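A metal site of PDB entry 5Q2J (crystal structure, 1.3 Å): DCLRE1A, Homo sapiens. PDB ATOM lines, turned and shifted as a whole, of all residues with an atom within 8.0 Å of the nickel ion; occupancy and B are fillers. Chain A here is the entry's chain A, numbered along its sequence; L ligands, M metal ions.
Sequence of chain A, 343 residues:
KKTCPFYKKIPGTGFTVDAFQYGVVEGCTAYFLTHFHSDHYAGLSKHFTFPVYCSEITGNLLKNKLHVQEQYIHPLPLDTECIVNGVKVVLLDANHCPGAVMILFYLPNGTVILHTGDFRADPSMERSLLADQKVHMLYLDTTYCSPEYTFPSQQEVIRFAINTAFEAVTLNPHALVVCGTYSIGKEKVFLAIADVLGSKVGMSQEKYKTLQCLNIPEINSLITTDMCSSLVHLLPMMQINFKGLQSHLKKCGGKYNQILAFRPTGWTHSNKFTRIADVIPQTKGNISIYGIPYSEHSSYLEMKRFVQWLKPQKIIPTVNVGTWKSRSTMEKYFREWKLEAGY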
ATOM      1  N   ASP A  18       2.389  -9.078  16.524  1.00  0.00           N
ATOM      2  CA  ASP A  18       2.523 -10.047  15.372  1.00  0.00           C
ATOM      3  C   ASP A  18       1.344  -9.828  14.318  1.00  0.00           C
ATOM      4  O   ASP A  18       0.660 -10.805  13.862  1.00  0.00           O
ATOM      5  CB  ASP A  18       2.627 -11.472  15.814  1.00  0.00           C
ATOM      6  CG  ASP A  18       3.872 -11.724  16.744  1.00  0.00           C
ATOM      7  OD1 ASP A  18       4.793 -10.814  16.796  1.00  0.00           O
ATOM      8  OD2 ASP A  18       3.880 -12.880  17.307  1.00  0.00           O
ATOM      9  N   THR A  34       7.225 -10.528  18.070  1.00  0.00           N
ATOM     10  CA  THR A  34       7.803 -11.480  19.059  1.00  0.00           C
ATOM     11  C   THR A  34       9.073 -12.190  18.548  1.00  0.00           C
ATOM     12  O   THR A  34       9.971 -12.424  19.352  1.00  0.00           O
ATOM     13  CB  THR A  34       6.816 -12.455  19.610  1.00  0.00           C
ATOM     14  OG1 THR A  34       6.294 -13.327  18.573  1.00  0.00           O
ATOM     15  CG2 THR A  34       5.601 -11.781  20.335  1.00  0.00           C
ATOM     16  N   HIS A  35       9.082 -12.592  17.254  1.00  0.00           N
ATOM     17  CA  HIS A  35      10.179 -13.382  16.670  1.00  0.00           C
ATOM     18  C   HIS A  35      10.119 -13.370  15.181  1.00  0.00           C
ATOM     19  O   HIS A  35       8.988 -13.168  14.612  1.00  0.00           O
ATOM     20  CB  HIS A  35      10.215 -14.792  17.340  1.00  0.00           C
ATOM     21  CG  HIS A  35       9.087 -15.731  17.020  1.00  0.00           C
ATOM     22  ND1 HIS A  35       7.769 -15.569  17.373  1.00  0.00           N
ATOM     23  CD2 HIS A  35       9.103 -16.873  16.294  1.00  0.00           C
ATOM     24  CE1 HIS A  35       7.074 -16.618  16.945  1.00  0.00           C
ATOM     25  NE2 HIS A  35       7.882 -17.430  16.334  1.00  0.00           N
ATOM     26  N   PHE A  36      11.201 -13.793  14.607  1.00  0.00           N
ATOM     27  CA  PHE A  36      11.358 -13.844  13.109  1.00  0.00           C
ATOM     28  C   PHE A  36      10.945 -15.195  12.497  1.00  0.00           C
ATOM     29  O   PHE A  36      11.846 -15.951  11.946  1.00  0.00           O
ATOM     30  CB  PHE A  36      12.797 -13.377  12.696  1.00  0.00           C
ATOM     31  CG  PHE A  36      12.971 -13.050  11.220  1.00  0.00           C
ATOM     32  CD1 PHE A  36      12.480 -11.834  10.706  1.00  0.00           C
ATOM     33  CD2 PHE A  36      13.619 -13.911  10.369  1.00  0.00           C
ATOM     34  CE1 PHE A  36      12.658 -11.543   9.332  1.00  0.00           C
ATOM     35  CE2 PHE A  36      13.758 -13.651   9.029  1.00  0.00           C
ATOM     36  CZ  PHE A  36      13.356 -12.456   8.512  1.00  0.00           C
ATOM     37  N   HIS A  37       9.659 -15.582  12.606  1.00  0.00           N
ATOM     38  CA  HIS A  37       9.047 -16.701  11.919  1.00  0.00           C
ATOM     39  C   HIS A  37       7.921 -16.139  10.977  1.00  0.00           C
ATOM     40  O   HIS A  37       7.148 -15.252  11.390  1.00  0.00           O
ATOM     41  CB  HIS A  37       8.473 -17.774  12.846  1.00  0.00           C
ATOM     42  CG  HIS A  37       9.506 -18.756  13.398  1.00  0.00           C
ATOM     43  ND1 HIS A  37       9.268 -19.560  14.505  1.00  0.00           N
ATOM     44  CD2 HIS A  37      10.751 -19.044  13.001  1.00  0.00           C
ATOM     45  CE1 HIS A  37      10.323 -20.341  14.714  1.00  0.00           C
ATOM     46  NE2 HIS A  37      11.217 -20.019  13.824  1.00  0.00           N
ATOM     47  N   SER A  38       7.835 -16.725   9.763  1.00  0.00           N
ATOM     48  CA  SER A  38       7.039 -16.083   8.698  1.00  0.00           C
ATOM     49  C   SER A  38       5.580 -15.950   8.998  1.00  0.00           C
ATOM     50  O   SER A  38       5.058 -14.902   8.603  1.00  0.00           O
ATOM     51  CB  SER A  38       7.341 -16.679   7.313  1.00  0.00           C
ATOM     52  OG  SER A  38       7.025 -18.035   7.285  1.00  0.00           O
ATOM     53  N   ASP A  39       4.946 -16.861   9.713  1.00  0.00           N
ATOM     54  CA  ASP A  39       3.493 -16.683  10.080  1.00  0.00           C
ATOM     55  C   ASP A  39       3.326 -15.413  10.947  1.00  0.00           C
ATOM     56  O   ASP A  39       2.237 -14.805  10.948  1.00  0.00           O
ATOM     57  CB  ASP A  39       2.860 -17.875  10.750  1.00  0.00           C
ATOM     58  CG  ASP A  39       2.474 -19.071   9.757  1.00  0.00           C
ATOM     59  OD1 ASP A  39       2.675 -18.934   8.522  1.00  0.00           O
ATOM     60  OD2 ASP A  39       2.030 -20.124  10.302  1.00  0.00           O
ATOM     61  N   HIS A  40       4.367 -15.019  11.685  1.00  0.00           N
ATOM     62  CA  HIS A  40       4.291 -13.878  12.621  1.00  0.00           C
ATOM     63  C   HIS A  40       4.696 -12.603  12.006  1.00  0.00           C
ATOM     64  O   HIS A  40       4.091 -11.546  12.320  1.00  0.00           O
ATOM     65  CB  HIS A  40       5.178 -14.189  13.886  1.00  0.00           C
ATOM     66  CG  HIS A  40       4.671 -15.351  14.644  1.00  0.00           C
ATOM     67  ND1 HIS A  40       3.890 -15.221  15.765  1.00  0.00           N
ATOM     68  CD2 HIS A  40       4.712 -16.688  14.389  1.00  0.00           C
ATOM     69  CE1 HIS A  40       3.482 -16.409  16.158  1.00  0.00           C
ATOM     70  NE2 HIS A  40       3.997 -17.325  15.365  1.00  0.00           N
ATOM     71  N   HIS A  96      12.446 -20.062  22.580  1.00  0.00           N
ATOM     72  CA  HIS A  96      11.926 -20.515  21.268  1.00  0.00           C
ATOM     73  C   HIS A  96      13.110 -20.518  20.291  1.00  0.00           C
ATOM     74  O   HIS A  96      14.064 -21.332  20.492  1.00  0.00           O
ATOM     75  CB  HIS A  96      10.706 -19.657  20.887  1.00  0.00           C
ATOM     76  CG  HIS A  96       9.964 -20.043  19.612  1.00  0.00           C
ATOM     77  ND1 HIS A  96       9.545 -21.309  19.326  1.00  0.00           N
ATOM     78  CD2 HIS A  96       9.656 -19.308  18.490  1.00  0.00           C
ATOM     79  CE1 HIS A  96       8.901 -21.324  18.150  1.00  0.00           C
ATOM     80  NE2 HIS A  96       8.953 -20.130  17.613  1.00  0.00           N
ATOM     81  N   CYS A  97      13.104 -19.714  19.257  1.00  0.00           N
ATOM     82  CA  CYS A  97      14.284 -19.568  18.344  1.00  0.00           C
ATOM     83  C   CYS A  97      15.112 -18.338  18.737  1.00  0.00           C
ATOM     84  O   CYS A  97      14.666 -17.547  19.592  1.00  0.00           O
ATOM     85  CB  CYS A  97      13.708 -19.404  16.868  1.00  0.00           C
ATOM     86  SG  CYS A  97      12.714 -17.871  16.632  1.00  0.00           S
ATOM     87  N   ALA A 100      13.690 -14.609  19.989  1.00  0.00           N
ATOM     88  CA  ALA A 100      12.230 -14.734  20.356  1.00  0.00           C
ATOM     89  C   ALA A 100      12.021 -14.265  21.798  1.00  0.00           C
ATOM     90  O   ALA A 100      12.762 -14.626  22.723  1.00  0.00           O
ATOM     91  CB  ALA A 100      11.713 -16.150  20.199  1.00  0.00           C
ATOM     92  N   GLY A 117       4.226 -14.859  22.985  1.00  0.00           N
ATOM     93  CA  GLY A 117       4.626 -15.231  21.614  1.00  0.00           C
ATOM     94  C   GLY A 117       4.625 -16.718  21.472  1.00  0.00           C
ATOM     95  O   GLY A 117       3.721 -17.421  21.979  1.00  0.00           O
ATOM     96  N   ASP A 118       5.584 -17.224  20.685  1.00  0.00           N
ATOM     97  CA  ASP A 118       5.873 -18.675  20.682  1.00  0.00           C
ATOM     98  C   ASP A 118       6.918 -18.952  21.808  1.00  0.00           C
ATOM     99  O   ASP A 118       7.912 -18.172  21.957  1.00  0.00           O
ATOM    100  CB  ASP A 118       6.406 -19.143  19.333  1.00  0.00           C
ATOM    101  CG  ASP A 118       5.338 -19.354  18.266  1.00  0.00           C
ATOM    102  OD1 ASP A 118       4.124 -19.293  18.537  1.00  0.00           O
ATOM    103  OD2 ASP A 118       5.747 -19.614  17.154  1.00  0.00           O
ATOM    104  N   PHE A 119       6.685 -19.990  22.583  1.00  0.00           N
ATOM    105  CA  PHE A 119       7.624 -20.316  23.719  1.00  0.00           C
ATOM    106  C   PHE A 119       7.693 -21.807  24.030  1.00  0.00           C
ATOM    107  O   PHE A 119       6.793 -22.572  23.717  1.00  0.00           O
ATOM    108  CB  PHE A 119       7.350 -19.459  25.004  1.00  0.00           C
ATOM    109  CG  PHE A 119       6.265 -19.962  26.010  1.00  0.00           C
ATOM    110  CD1 PHE A 119       6.479 -19.850  27.392  1.00  0.00           C
ATOM    111  CD2 PHE A 119       5.006 -20.483  25.606  1.00  0.00           C
ATOM    112  CE1 PHE A 119       5.487 -20.212  28.324  1.00  0.00           C
ATOM    113  CE2 PHE A 119       4.050 -20.907  26.529  1.00  0.00           C
ATOM    114  CZ  PHE A 119       4.319 -20.780  27.867  1.00  0.00           C
ATOM    115  N   ASP A 141       0.768 -19.380  23.914  1.00  0.00           N
ATOM    116  CA  ASP A 141       1.117 -20.315  22.808  1.00  0.00           C
ATOM    117  C   ASP A 141       0.670 -21.689  23.213  1.00  0.00           C
ATOM    118  O   ASP A 141       1.251 -22.403  24.059  1.00  0.00           O
ATOM    119  CB  ASP A 141       2.633 -20.312  22.588  1.00  0.00           C
ATOM    120  CG  ASP A 141       3.119 -21.433  21.675  1.00  0.00           C
ATOM    121  OD1 ASP A 141       2.240 -22.077  20.991  1.00  0.00           O
ATOM    122  OD2 ASP A 141       4.336 -21.660  21.648  1.00  0.00           O
ATOM    123  N   THR A 143       0.176 -24.353  21.056  1.00  0.00           N
ATOM    124  CA  THR A 143       0.474 -25.258  19.922  1.00  0.00           C
ATOM    125  C   THR A 143       0.239 -26.689  20.335  1.00  0.00           C
ATOM    126  O   THR A 143      -0.536 -27.400  19.552  1.00  0.00           O
ATOM    127  CB  THR A 143       1.955 -25.035  19.452  1.00  0.00           C
ATOM    128  OG1 THR A 143       2.136 -23.732  18.918  1.00  0.00           O
ATOM    129  CG2 THR A 143       2.356 -26.031  18.375  1.00  0.00           C
ATOM    130  N   SER A 183      13.745 -22.336   8.447  1.00  0.00           N
ATOM    131  CA  SER A 183      13.486 -21.120   9.187  1.00  0.00           C
ATOM    132  C   SER A 183      14.639 -21.052  10.191  1.00  0.00           C
ATOM    133  O   SER A 183      15.410 -22.039  10.338  1.00  0.00           O
ATOM    134  CB  SER A 183      12.150 -21.195   9.986  1.00  0.00           C
ATOM    135  OG  SER A 183      12.161 -22.310  10.897  1.00  0.00           O
ATOM    136  N   ILE A 184      14.758 -19.945  10.892  1.00  0.00           N
ATOM    137  CA  ILE A 184      15.614 -19.925  12.093  1.00  0.00           C
ATOM    138  C   ILE A 184      15.040 -20.777  13.250  1.00  0.00           C
ATOM    139  O   ILE A 184      13.823 -21.126  13.264  1.00  0.00           O
ATOM    140  CB  ILE A 184      15.932 -18.497  12.619  1.00  0.00           C
ATOM    141  CG1 ILE A 184      14.697 -17.786  13.140  1.00  0.00           C
ATOM    142  CG2 ILE A 184      16.605 -17.691  11.505  1.00  0.00           C
ATOM    143  CD1 ILE A 184      14.983 -16.573  14.004  1.00  0.00           C
ATOM    144  N   GLU A 296      10.755 -26.640  19.756  1.00  0.00           N
ATOM    145  CA  GLU A 296      10.876 -25.278  20.339  1.00  0.00           C
ATOM    146  C   GLU A 296       9.536 -24.673  20.889  1.00  0.00           C
ATOM    147  O   GLU A 296       9.366 -23.470  21.093  1.00  0.00           O
ATOM    148  CB  GLU A 296      11.632 -24.319  19.448  1.00  0.00           C
ATOM    149  CG  GLU A 296      13.160 -24.721  19.378  1.00  0.00           C
ATOM    150  CD  GLU A 296      14.031 -23.753  18.549  1.00  0.00           C
ATOM    151  OE1 GLU A 296      13.533 -22.967  17.695  1.00  0.00           O
ATOM    152  OE2 GLU A 296      15.310 -23.837  18.763  1.00  0.00           O
ATOM    153  N   HIS A 297       8.582 -25.592  21.092  1.00  0.00           N
ATOM    154  CA  HIS A 297       7.283 -25.238  21.764  1.00  0.00           C
ATOM    155  C   HIS A 297       7.107 -26.126  22.998  1.00  0.00           C
ATOM    156  O   HIS A 297       7.599 -27.282  23.061  1.00  0.00           O
ATOM    157  CB  HIS A 297       6.063 -25.475  20.868  1.00  0.00           C
ATOM    158  CG  HIS A 297       5.960 -24.592  19.660  1.00  0.00           C
ATOM    159  ND1 HIS A 297       5.382 -23.336  19.653  1.00  0.00           N
ATOM    160  CD2 HIS A 297       6.317 -24.840  18.359  1.00  0.00           C
ATOM    161  CE1 HIS A 297       5.471 -22.813  18.437  1.00  0.00           C
ATOM    162  NE2 HIS A 297       6.020 -23.717  17.642  1.00  0.00           N
HETATM  163  C1  LIG L   1       6.468 -21.596  13.414  1.00  0.00           C
HETATM  164  C2  LIG L   1       6.741 -22.331  14.728  1.00  0.00           C
HETATM  165  C3  LIG L   1       5.781 -20.245  13.646  1.00  0.00           C
HETATM  166  O1  LIG L   1       6.507 -23.504  14.871  1.00  0.00           O
HETATM  167  O2  LIG L   1       7.262 -21.709  15.653  1.00  0.00           O
HETATM  168  O3  LIG L   1       6.273 -19.389  14.454  1.00  0.00           O
HETATM  169  O4  LIG L   1       4.844 -19.960  12.842  1.00  0.00           O
HETATM  170 NI    NI M   1       7.609 -19.591  15.942  1.00  0.00          NI
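A ring nitrogen (NE2) of His 37 lies within hydrogen-bond range of the backbone carbonyl oxygen (O) of Ile 184.
The backbone carbonyl oxygen (O) of Glu 296 sits at hydrogen-bond distance from a ring nitrogen (ND1) of His 96, 2.8 Å away.
A ring nitrogen (ND1) of His 35 is in hydrogen-bond range of the side-chain hydroxyl of Thr 34.
A ring nitrogen (NE2) of His 40 lies close to the side-chain carboxylate (OD2) of Asp 118 (3.4 Å).
The nickel ion is bound by O3 of the ligand (2.0 Å), O2 of the ligand (2.2 Å), ND1 of His 37 (2.2 Å), NE2 of His 96 (2.2 Å), NE2 of His 35 (2.2 Å) and OD2 of Asp 118 (2.2 Å).
The nickel ion has six donor atoms within binding distance.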
